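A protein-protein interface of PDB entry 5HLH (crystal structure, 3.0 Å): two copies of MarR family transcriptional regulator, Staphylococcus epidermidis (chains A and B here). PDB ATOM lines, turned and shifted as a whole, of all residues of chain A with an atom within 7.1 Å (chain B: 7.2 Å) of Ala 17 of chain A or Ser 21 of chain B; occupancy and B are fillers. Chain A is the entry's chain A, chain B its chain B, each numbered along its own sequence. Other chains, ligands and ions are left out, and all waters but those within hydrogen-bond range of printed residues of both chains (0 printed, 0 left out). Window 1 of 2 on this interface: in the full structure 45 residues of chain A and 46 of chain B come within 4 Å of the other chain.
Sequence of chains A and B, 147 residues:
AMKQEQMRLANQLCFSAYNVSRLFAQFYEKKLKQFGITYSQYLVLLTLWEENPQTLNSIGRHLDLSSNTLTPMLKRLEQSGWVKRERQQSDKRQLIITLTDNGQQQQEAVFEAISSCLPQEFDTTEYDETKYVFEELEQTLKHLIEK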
ATOM      1  N   GLN A  12      26.566 -10.372  -9.217  1.00  0.00           N
ATOM      2  CA  GLN A  12      27.663 -11.321  -8.906  1.00  0.00           C
ATOM      3  C   GLN A  12      27.900 -11.556  -7.422  1.00  0.00           C
ATOM      4  O   GLN A  12      28.745 -12.374  -7.078  1.00  0.00           O
ATOM      5  CB  GLN A  12      28.959 -11.064  -9.691  1.00  0.00           C
ATOM      6  CG  GLN A  12      29.700  -9.768  -9.439  1.00  0.00           C
ATOM      7  CD  GLN A  12      30.633  -9.407 -10.617  1.00  0.00           C
ATOM      8  OE1 GLN A  12      31.235 -10.290 -11.238  1.00  0.00           O
ATOM      9  NE2 GLN A  12      30.724  -8.107 -10.949  1.00  0.00           N
ATOM     10  N   LEU A  13      27.114 -10.898  -6.560  1.00  0.00           N
ATOM     11  CA  LEU A  13      27.019 -11.248  -5.130  1.00  0.00           C
ATOM     12  C   LEU A  13      25.903 -12.213  -4.744  1.00  0.00           C
ATOM     13  O   LEU A  13      26.146 -13.054  -3.882  1.00  0.00           O
ATOM     14  CB  LEU A  13      26.855 -10.005  -4.270  1.00  0.00           C
ATOM     15  CG  LEU A  13      28.094  -9.183  -3.952  1.00  0.00           C
ATOM     16  CD1 LEU A  13      27.693  -7.986  -3.106  1.00  0.00           C
ATOM     17  CD2 LEU A  13      29.151 -10.000  -3.215  1.00  0.00           C
ATOM     18  N   OCS A  14      24.679 -12.066  -5.287  1.00  0.00           N
ATOM     19  CA  OCS A  14      23.614 -13.112  -5.136  1.00  0.00           C
ATOM     20  CB  OCS A  14      22.295 -12.925  -5.980  1.00  0.00           C
ATOM     21  SG  OCS A  14      21.291 -14.249  -6.441  1.00  0.00           S
ATOM     22  C   OCS A  14      24.386 -14.347  -5.501  1.00  0.00           C
ATOM     23  O   OCS A  14      24.562 -15.240  -4.662  1.00  0.00           O
ATOM     24  OD1 OCS A  14      20.237 -14.554  -5.495  1.00  0.00           O
ATOM     25  OD2 OCS A  14      20.730 -14.088  -7.760  1.00  0.00           O
ATOM     26  OD3 OCS A  14      22.128 -15.625  -6.592  1.00  0.00           O
ATOM     27  N   PHE A  15      24.927 -14.355  -6.724  1.00  0.00           N
ATOM     28  CA  PHE A  15      25.449 -15.566  -7.337  1.00  0.00           C
ATOM     29  C   PHE A  15      26.592 -16.162  -6.566  1.00  0.00           C
ATOM     30  O   PHE A  15      26.597 -17.341  -6.288  1.00  0.00           O
ATOM     31  CB  PHE A  15      25.851 -15.316  -8.788  1.00  0.00           C
ATOM     32  CG  PHE A  15      26.202 -16.563  -9.552  1.00  0.00           C
ATOM     33  CD1 PHE A  15      25.442 -17.715  -9.436  1.00  0.00           C
ATOM     34  CD2 PHE A  15      27.268 -16.571 -10.416  1.00  0.00           C
ATOM     35  CE1 PHE A  15      25.757 -18.852 -10.152  1.00  0.00           C
ATOM     36  CE2 PHE A  15      27.587 -17.693 -11.137  1.00  0.00           C
ATOM     37  CZ  PHE A  15      26.833 -18.835 -11.006  1.00  0.00           C
ATOM     38  N   SER A  16      27.551 -15.337  -6.199  1.00  0.00           N
ATOM     39  CA  SER A  16      28.650 -15.805  -5.363  1.00  0.00           C
ATOM     40  C   SER A  16      28.170 -16.437  -4.018  1.00  0.00           C
ATOM     41  O   SER A  16      28.577 -17.545  -3.685  1.00  0.00           O
ATOM     42  CB  SER A  16      29.642 -14.666  -5.117  1.00  0.00           C
ATOM     43  OG  SER A  16      30.870 -15.176  -4.626  1.00  0.00           O
ATOM     44  N   ALA A  17      27.291 -15.746  -3.276  1.00  0.00           N
ATOM     45  CA  ALA A  17      26.749 -16.251  -1.995  1.00  0.00           C
ATOM     46  C   ALA A  17      25.908 -17.509  -2.201  1.00  0.00           C
ATOM     47  O   ALA A  17      25.907 -18.414  -1.357  1.00  0.00           O
ATOM     48  CB  ALA A  17      25.934 -15.169  -1.298  1.00  0.00           C
ATOM     49  N   TYR A  18      25.213 -17.545  -3.340  1.00  0.00           N
ATOM     50  CA  TYR A  18      24.442 -18.700  -3.769  1.00  0.00           C
ATOM     51  C   TYR A  18      25.311 -19.896  -4.007  1.00  0.00           C
ATOM     52  O   TYR A  18      24.905 -20.990  -3.666  1.00  0.00           O
ATOM     53  CB  TYR A  18      23.664 -18.373  -5.040  1.00  0.00           C
ATOM     54  CG  TYR A  18      22.922 -19.515  -5.725  1.00  0.00           C
ATOM     55  CD1 TYR A  18      21.843 -20.160  -5.102  1.00  0.00           C
ATOM     56  CD2 TYR A  18      23.271 -19.907  -7.021  1.00  0.00           C
ATOM     57  CE1 TYR A  18      21.159 -21.170  -5.737  1.00  0.00           C
ATOM     58  CE2 TYR A  18      22.599 -20.928  -7.665  1.00  0.00           C
ATOM     59  CZ  TYR A  18      21.545 -21.543  -7.023  1.00  0.00           C
ATOM     60  OH  TYR A  18      20.866 -22.526  -7.677  1.00  0.00           O
ATOM     61  N   ASN A  19      26.490 -19.713  -4.593  1.00  0.00           N
ATOM     62  CA  ASN A  19      27.450 -20.827  -4.722  1.00  0.00           C
ATOM     63  C   ASN A  19      28.031 -21.282  -3.350  1.00  0.00           C
ATOM     64  O   ASN A  19      28.067 -22.473  -3.030  1.00  0.00           O
ATOM     65  CB  ASN A  19      28.562 -20.459  -5.714  1.00  0.00           C
ATOM     66  CG  ASN A  19      28.073 -20.396  -7.155  1.00  0.00           C
ATOM     67  OD1 ASN A  19      27.231 -21.187  -7.574  1.00  0.00           O
ATOM     68  ND2 ASN A  19      28.634 -19.473  -7.933  1.00  0.00           N
ATOM     69  N   VAL A  20      28.440 -20.321  -2.530  1.00  0.00           N
ATOM     70  CA  VAL A  20      29.155 -20.616  -1.302  1.00  0.00           C
ATOM     71  C   VAL A  20      28.325 -21.454  -0.346  1.00  0.00           C
ATOM     72  O   VAL A  20      28.838 -22.408   0.252  1.00  0.00           O
ATOM     73  CB  VAL A  20      29.631 -19.316  -0.615  1.00  0.00           C
ATOM     74  CG1 VAL A  20      30.092 -19.566   0.820  1.00  0.00           C
ATOM     75  CG2 VAL A  20      30.767 -18.701  -1.411  1.00  0.00           C
ATOM     76  N   SER A  21      27.061 -21.088  -0.176  1.00  0.00           N
ATOM     77  CA  SER A  21      26.180 -21.845   0.720  1.00  0.00           C
ATOM     78  C   SER A  21      25.893 -23.249   0.205  1.00  0.00           C
ATOM     79  O   SER A  21      25.758 -24.174   1.000  1.00  0.00           O
ATOM     80  CB  SER A  21      24.862 -21.115   0.940  1.00  0.00           C
ATOM     81  OG  SER A  21      24.116 -21.046  -0.267  1.00  0.00           O
ATOM     82  N   ARG A  22      25.794 -23.397  -1.119  1.00  0.00           N
ATOM     83  CA  ARG A  22      25.664 -24.725  -1.749  1.00  0.00           C
ATOM     84  C   ARG A  22      26.878 -25.606  -1.488  1.00  0.00           C
ATOM     85  O   ARG A  22      26.722 -26.748  -1.072  1.00  0.00           O
ATOM     86  CB  ARG A  22      25.448 -24.625  -3.262  1.00  0.00           C
ATOM     87  CG  ARG A  22      24.001 -24.509  -3.685  1.00  0.00           C
ATOM     88  CD  ARG A  22      23.857 -23.725  -4.968  1.00  0.00           C
ATOM     89  NE  ARG A  22      24.201 -24.497  -6.154  1.00  0.00           N
ATOM     90  CZ  ARG A  22      24.773 -24.010  -7.265  1.00  0.00           C
ATOM     91  NH1 ARG A  22      25.137 -22.743  -7.396  1.00  0.00           N
ATOM     92  NH2 ARG A  22      25.009 -24.823  -8.271  1.00  0.00           N
ATOM     93  N   LEU A  23      28.083 -25.058  -1.703  1.00  0.00           N
ATOM     94  CA  LEU A  23      29.358 -25.810  -1.496  1.00  0.00           C
ATOM     95  C   LEU A  23      29.575 -26.229  -0.043  1.00  0.00           C
ATOM     96  O   LEU A  23      29.864 -27.382   0.222  1.00  0.00           O
ATOM     97  CB  LEU A  23      30.574 -25.031  -2.028  1.00  0.00           C
ATOM     98  CG  LEU A  23      30.558 -24.796  -3.551  1.00  0.00           C
ATOM     99  CD1 LEU A  23      31.456 -23.659  -3.993  1.00  0.00           C
ATOM    100  CD2 LEU A  23      30.942 -26.054  -4.291  1.00  0.00           C
ATOM    101  N   PHE A 134      30.949 -11.008   5.839  1.00  0.00           N
ATOM    102  CA  PHE A 134      29.684 -11.737   5.785  1.00  0.00           C
ATOM    103  C   PHE A 134      28.721 -11.061   6.760  1.00  0.00           C
ATOM    104  O   PHE A 134      27.720 -10.459   6.327  1.00  0.00           O
ATOM    105  CB  PHE A 134      29.876 -13.245   6.079  1.00  0.00           C
ATOM    106  CG  PHE A 134      30.285 -14.079   4.854  1.00  0.00           C
ATOM    107  CD1 PHE A 134      31.556 -13.955   4.286  1.00  0.00           C
ATOM    108  CD2 PHE A 134      29.406 -15.001   4.288  1.00  0.00           C
ATOM    109  CE1 PHE A 134      31.927 -14.706   3.178  1.00  0.00           C
ATOM    110  CE2 PHE A 134      29.777 -15.752   3.184  1.00  0.00           C
ATOM    111  CZ  PHE A 134      31.040 -15.607   2.633  1.00  0.00           C
ATOM    112  N   LEU A 137      27.264  -7.755   5.529  1.00  0.00           N
ATOM    113  CA  LEU A 137      26.332  -7.932   4.391  1.00  0.00           C
ATOM    114  C   LEU A 137      25.002  -8.544   4.862  1.00  0.00           C
ATOM    115  O   LEU A 137      23.921  -8.178   4.366  1.00  0.00           O
ATOM    116  CB  LEU A 137      26.963  -8.810   3.303  1.00  0.00           C
ATOM    117  CG  LEU A 137      26.148  -9.065   2.026  1.00  0.00           C
ATOM    118  CD1 LEU A 137      25.781  -7.798   1.273  1.00  0.00           C
ATOM    119  CD2 LEU A 137      26.922 -10.021   1.124  1.00  0.00           C
ATOM    120  N   LEU A 141      21.503  -6.632   4.228  1.00  0.00           N
ATOM    121  CA  LEU A 141      20.353  -7.288   3.598  1.00  0.00           C
ATOM    122  C   LEU A 141      19.107  -7.279   4.516  1.00  0.00           C
ATOM    123  O   LEU A 141      17.983  -7.043   4.030  1.00  0.00           O
ATOM    124  CB  LEU A 141      20.712  -8.713   3.145  1.00  0.00           C
ATOM    125  CG  LEU A 141      21.584  -8.893   1.880  1.00  0.00           C
ATOM    126  CD1 LEU A 141      21.452 -10.312   1.340  1.00  0.00           C
ATOM    127  CD2 LEU A 141      21.239  -7.912   0.766  1.00  0.00           C
ATOM    128  N   SER B  16      26.805 -18.304   8.534  1.00  0.00           N
ATOM    129  CA  SER B  16      26.760 -16.948   8.005  1.00  0.00           C
ATOM    130  C   SER B  16      26.458 -16.849   6.492  1.00  0.00           C
ATOM    131  O   SER B  16      25.786 -15.908   6.070  1.00  0.00           O
ATOM    132  CB  SER B  16      28.066 -16.235   8.305  1.00  0.00           C
ATOM    133  OG  SER B  16      27.857 -14.851   8.109  1.00  0.00           O
ATOM    134  N   ALA B  17      26.999 -17.784   5.691  1.00  0.00           N
ATOM    135  CA  ALA B  17      26.747 -17.860   4.227  1.00  0.00           C
ATOM    136  C   ALA B  17      25.368 -18.439   3.937  1.00  0.00           C
ATOM    137  O   ALA B  17      24.733 -18.107   2.926  1.00  0.00           O
ATOM    138  CB  ALA B  17      27.813 -18.704   3.538  1.00  0.00           C
ATOM    139  N   TYR B  18      24.931 -19.327   4.825  1.00  0.00           N
ATOM    140  CA  TYR B  18      23.574 -19.859   4.820  1.00  0.00           C
ATOM    141  C   TYR B  18      22.563 -18.734   4.989  1.00  0.00           C
ATOM    142  O   TYR B  18      21.640 -18.628   4.182  1.00  0.00           O
ATOM    143  CB  TYR B  18      23.428 -20.906   5.918  1.00  0.00           C
ATOM    144  CG  TYR B  18      22.054 -21.499   6.152  1.00  0.00           C
ATOM    145  CD1 TYR B  18      21.418 -22.285   5.185  1.00  0.00           C
ATOM    146  CD2 TYR B  18      21.424 -21.355   7.380  1.00  0.00           C
ATOM    147  CE1 TYR B  18      20.169 -22.863   5.433  1.00  0.00           C
ATOM    148  CE2 TYR B  18      20.189 -21.935   7.637  1.00  0.00           C
ATOM    149  CZ  TYR B  18      19.563 -22.669   6.664  1.00  0.00           C
ATOM    150  OH  TYR B  18      18.335 -23.192   6.938  1.00  0.00           O
ATOM    151  N   ASN B  19      22.765 -17.856   5.970  1.00  0.00           N
ATOM    152  CA  ASN B  19      21.888 -16.695   6.134  1.00  0.00           C
ATOM    153  C   ASN B  19      21.955 -15.693   4.956  1.00  0.00           C
ATOM    154  O   ASN B  19      20.938 -15.166   4.539  1.00  0.00           O
ATOM    155  CB  ASN B  19      22.165 -15.979   7.465  1.00  0.00           C
ATOM    156  CG  ASN B  19      21.873 -16.849   8.700  1.00  0.00           C
ATOM    157  OD1 ASN B  19      21.054 -17.765   8.682  1.00  0.00           O
ATOM    158  ND2 ASN B  19      22.561 -16.550   9.788  1.00  0.00           N
ATOM    159  N   VAL B  20      23.131 -15.438   4.409  1.00  0.00           N
ATOM    160  CA  VAL B  20      23.283 -14.418   3.358  1.00  0.00           C
ATOM    161  C   VAL B  20      22.625 -14.799   2.025  1.00  0.00           C
ATOM    162  O   VAL B  20      22.023 -13.960   1.350  1.00  0.00           O
ATOM    163  CB  VAL B  20      24.779 -14.110   3.116  1.00  0.00           C
ATOM    164  CG1 VAL B  20      25.003 -13.327   1.822  1.00  0.00           C
ATOM    165  CG2 VAL B  20      25.330 -13.336   4.293  1.00  0.00           C
ATOM    166  N   SER B  21      22.792 -16.060   1.639  1.00  0.00           N
ATOM    167  CA  SER B  21      22.159 -16.600   0.438  1.00  0.00           C
ATOM    168  C   SER B  21      20.637 -16.557   0.543  1.00  0.00           C
ATOM    169  O   SER B  21      19.956 -16.129  -0.409  1.00  0.00           O
ATOM    170  CB  SER B  21      22.601 -18.043   0.216  1.00  0.00           C
ATOM    171  OG  SER B  21      21.998 -18.583  -0.954  1.00  0.00           O
ATOM    172  N   ARG B  22      20.118 -16.991   1.702  1.00  0.00           N
ATOM    173  CA  ARG B  22      18.665 -16.879   2.003  1.00  0.00           C
ATOM    174  C   ARG B  22      18.134 -15.452   1.845  1.00  0.00           C
ATOM    175  O   ARG B  22      17.218 -15.216   1.062  1.00  0.00           O
ATOM    176  CB  ARG B  22      18.319 -17.403   3.402  1.00  0.00           C
ATOM    177  CG  ARG B  22      18.017 -18.893   3.431  1.00  0.00           C
ATOM    178  CD  ARG B  22      18.336 -19.513   4.771  1.00  0.00           C
ATOM    179  NE  ARG B  22      17.416 -19.102   5.813  1.00  0.00           N
ATOM    180  CZ  ARG B  22      17.732 -18.951   7.098  1.00  0.00           C
ATOM    181  NH1 ARG B  22      18.968 -19.124   7.548  1.00  0.00           N
ATOM    182  NH2 ARG B  22      16.790 -18.591   7.956  1.00  0.00           N
ATOM    183  N   LEU B  23      18.737 -14.508   2.552  1.00  0.00           N
ATOM    184  CA  LEU B  23      18.326 -13.114   2.467  1.00  0.00           C
ATOM    185  C   LEU B  23      18.337 -12.529   1.048  1.00  0.00           C
ATOM    186  O   LEU B  23      17.462 -11.762   0.693  1.00  0.00           O
ATOM    187  CB  LEU B  23      19.204 -12.273   3.385  1.00  0.00           C
ATOM    188  CG  LEU B  23      19.094 -12.575   4.900  1.00  0.00           C
ATOM    189  CD1 LEU B  23      20.217 -11.861   5.643  1.00  0.00           C
ATOM    190  CD2 LEU B  23      17.728 -12.188   5.455  1.00  0.00           C
ATOM    191  N   PHE B  24      19.315 -12.892   0.234  1.00  0.00           N
ATOM    192  CA  PHE B  24      19.372 -12.406  -1.152  1.00  0.00           C
ATOM    193  C   PHE B  24      18.270 -12.994  -1.968  1.00  0.00           C
ATOM    194  O   PHE B  24      17.716 -12.327  -2.844  1.00  0.00           O
ATOM    195  CB  PHE B  24      20.658 -12.821  -1.847  1.00  0.00           C
ATOM    196  CG  PHE B  24      21.697 -11.751  -1.909  1.00  0.00           C
ATOM    197  CD1 PHE B  24      21.447 -10.550  -2.587  1.00  0.00           C
ATOM    198  CD2 PHE B  24      22.953 -11.945  -1.332  1.00  0.00           C
ATOM    199  CE1 PHE B  24      22.429  -9.548  -2.674  1.00  0.00           C
ATOM    200  CE2 PHE B  24      23.922 -10.957  -1.404  1.00  0.00           C
ATOM    201  CZ  PHE B  24      23.665  -9.762  -2.080  1.00  0.00           C
ATOM    202  N   ALA B  25      18.003 -14.276  -1.730  1.00  0.00           N
ATOM    203  CA  ALA B  25      16.913 -14.940  -2.433  1.00  0.00           C
ATOM    204  C   ALA B  25      15.604 -14.191  -2.088  1.00  0.00           C
ATOM    205  O   ALA B  25      14.873 -13.753  -3.002  1.00  0.00           O
ATOM    206  CB  ALA B  25      16.849 -16.415  -2.059  1.00  0.00           C
ATOM    207  N   GLN B  26      15.379 -13.983  -0.778  1.00  0.00           N
ATOM    208  CA  GLN B  26      14.222 -13.223  -0.283  1.00  0.00           C
ATOM    209  C   GLN B  26      14.134 -11.889  -1.014  1.00  0.00           C
ATOM    210  O   GLN B  26      13.089 -11.550  -1.579  1.00  0.00           O
ATOM    211  CB  GLN B  26      14.279 -12.979   1.233  1.00  0.00           C
ATOM    212  CG  GLN B  26      13.688 -14.074   2.102  1.00  0.00           C
ATOM    213  CD  GLN B  26      14.124 -13.998   3.562  1.00  0.00           C
ATOM    214  OE1 GLN B  26      14.908 -14.813   4.020  1.00  0.00           O
ATOM    215  NE2 GLN B  26      13.618 -13.018   4.294  1.00  0.00           N
ATOM    216  N   PHE B  27      15.236 -11.156  -1.039  1.00  0.00           N
ATOM    217  CA  PHE B  27      15.232  -9.855  -1.665  1.00  0.00           C
ATOM    218  C   PHE B  27      14.889  -9.927  -3.150  1.00  0.00           C
ATOM    219  O   PHE B  27      14.080  -9.160  -3.614  1.00  0.00           O
ATOM    220  CB  PHE B  27      16.565  -9.145  -1.466  1.00  0.00           C
ATOM    221  CG  PHE B  27      16.706  -7.907  -2.307  1.00  0.00           C
ATOM    222  CD1 PHE B  27      15.778  -6.875  -2.192  1.00  0.00           C
ATOM    223  CD2 PHE B  27      17.741  -7.781  -3.242  1.00  0.00           C
ATOM    224  CE1 PHE B  27      15.885  -5.740  -2.986  1.00  0.00           C
ATOM    225  CE2 PHE B  27      17.850  -6.645  -4.034  1.00  0.00           C
ATOM    226  CZ  PHE B  27      16.920  -5.623  -3.907  1.00  0.00           C
ATOM    227  N   TYR B  39      13.938 -16.542  -8.219  1.00  0.00           N
ATOM    228  CA  TYR B  39      15.377 -16.176  -8.341  1.00  0.00           C
ATOM    229  C   TYR B  39      16.222 -17.186  -9.148  1.00  0.00           C
ATOM    230  O   TYR B  39      17.037 -16.780  -9.968  1.00  0.00           O
ATOM    231  CB  TYR B  39      16.014 -15.893  -6.980  1.00  0.00           C
ATOM    232  CG  TYR B  39      16.060 -17.050  -6.028  1.00  0.00           C
ATOM    233  CD1 TYR B  39      14.975 -17.358  -5.239  1.00  0.00           C
ATOM    234  CD2 TYR B  39      17.195 -17.822  -5.905  1.00  0.00           C
ATOM    235  CE1 TYR B  39      14.994 -18.407  -4.361  1.00  0.00           C
ATOM    236  CE2 TYR B  39      17.231 -18.883  -5.013  1.00  0.00           C
ATOM    237  CZ  TYR B  39      16.115 -19.155  -4.246  1.00  0.00           C
ATOM    238  OH  TYR B  39      16.100 -20.164  -3.348  1.00  0.00           O
ATOM    239  N   PHE B 134      34.363 -13.306  -1.208  1.00  0.00           N
ATOM    240  CA  PHE B 134      33.461 -14.398  -1.575  1.00  0.00           C
ATOM    241  C   PHE B 134      34.097 -15.249  -2.666  1.00  0.00           C
ATOM    242  O   PHE B 134      34.337 -16.433  -2.436  1.00  0.00           O
ATOM    243  CB  PHE B 134      32.081 -13.883  -2.012  1.00  0.00           C
ATOM    244  CG  PHE B 134      31.149 -13.584  -0.862  1.00  0.00           C
ATOM    245  CD1 PHE B 134      31.352 -12.486  -0.045  1.00  0.00           C
ATOM    246  CD2 PHE B 134      30.069 -14.406  -0.600  1.00  0.00           C
ATOM    247  CE1 PHE B 134      30.498 -12.214   1.004  1.00  0.00           C
ATOM    248  CE2 PHE B 134      29.204 -14.136   0.445  1.00  0.00           C
ATOM    249  CZ  PHE B 134      29.423 -13.042   1.252  1.00  0.00           C
ATOM    250  N   GLU B 138      34.717 -19.283  -2.237  1.00  0.00           N
ATOM    251  CA  GLU B 138      34.132 -20.128  -3.283  1.00  0.00           C
ATOM    252  C   GLU B 138      35.208 -21.097  -3.731  1.00  0.00           C
ATOM    253  O   GLU B 138      35.080 -22.296  -3.502  1.00  0.00           O
ATOM    254  CB  GLU B 138      33.616 -19.240  -4.438  1.00  0.00           C
ATOM    255  CG  GLU B 138      32.672 -19.876  -5.447  1.00  0.00           C
ATOM    256  CD  GLU B 138      31.996 -18.849  -6.379  1.00  0.00           C
ATOM    257  OE1 GLU B 138      32.066 -17.618  -6.125  1.00  0.00           O
ATOM    258  OE2 GLU B 138      31.379 -19.277  -7.389  1.00  0.00           O
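OG of Ser 21 of chain A lies within hydrogen-bond range of OG of Ser 21 of chain B, at 3.3 Å. The side-chain carboxylate of Glu 138 of chain B lies within hydrogen-bond range of the side-chain hydroxyl of Ser 16 of chain A (3.1 Å). ND2 of Asn 19 of chain A is in hydrogen-bond range of OE2 of Glu 138 of chain B (2.8 Å).
The side-chain amide nitrogen (ND2) of Asn 19 of chain A is in hydrogen-bond range of the backbone carbonyl oxygen (O) of Phe 15 of chain A (3.4 Å). The guanidinium group of Arg 22 of chain A lies within hydrogen-bond range of the side-chain amide oxygen of Asn 19 of chain A (2.6 Å). O of Tyr 18 of chain A sits at hydrogen-bond distance from OG of Ser 21 of chain A, 3.5 Å away. O of Ala 17 of chain A lies within hydrogen-bond range of OG of Ser 21 of chain A, at 3.4 Å.
Leu 13 of chain A touches Phe 24 of chain B. Ser 16 of chain A touches Phe 134 of chain B (OG to CB, 3.2 Å). Val 20 of chain B touches Ala 17 of chain A. Phe 134 of chain B touches Ala 17 of chain A. Val 20 of chain A touches Ala 17 of chain B (CG1 to CB, 3.7 Å). Ser 16 of chain B touches Phe 134 of chain A. Phe 134 of chain A touches Ala 17 of chain B. CE2 of Phe 134 of chain B touches CZ of Phe 134 of chain A, at 3.2 Å. Leu 141 of chain A touches Val 20 of chain B (CD1 to O, 3.7 Å). CD2 of Phe 24 of chain B touches CD1 of Leu 141 of chain A, 3.5 Å away.
Printed residues of chain B within 4 Å of OCS 14 of chain A: Phe 24. Of chain B, only Val 20 (3.7 Å), Ser 21 (3.7 Å) and Phe 134 (3.8 Å) come within 4 Å of Ala 17 of chain A. Printed residues of chain B within 4 Å of Tyr 18 of chain A: Ser 21 (3.7 Å). Printed residues of chain B within 4 Å of Leu 137 of chain A: Val 20 (3.9 Å) and Phe 134 (3.9 Å). Ser 21 of chain B touches three residues of chain A. Of the printed residues of chain A, Leu 23 of chain B touches Leu 141. Of the printed residues of chain A, Phe 24 of chain B touches Leu 13 (3.9 Å), OCS 14 (3.99 Å) and Leu 141 (3.5 Å). The nearest residue of chain A that does not touch Ser 21 of chain B is OCS 14 of chain A (5.3 Å).
Hydrophobic or aromatic side chains of chain A that line the printed part of chain B: Leu 13, Ala 17, Val 20, Leu 23, Phe 134, Leu 137 and Leu 141. Among the printed residues, 21 pairs touch across the chains. Among the printed residues, no Asp or Glu carboxylate lies within 4 Å of a Lys or Arg side-chain nitrogen of the other chain.
Ser 16 of chain A touches Phe 134 of chain B, and with the chains exchanged Phe 134 of chain A touches Ser 16 of chain B. Ala 17 of chain A touches Val 20 of chain B, and with the chains exchanged Val 20 of chain A touches Ala 17 of chain B. Ala 17 of chain A touches Phe 134 of chain B, and with the chains exchanged Phe 134 of chain A touches Ala 17 of chain B. Tyr 18 of chain A touches Ser 21 of chain B, but with the chains exchanged Ser 21 of chain A does not touch Tyr 18 of chain B (4.3 Å).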
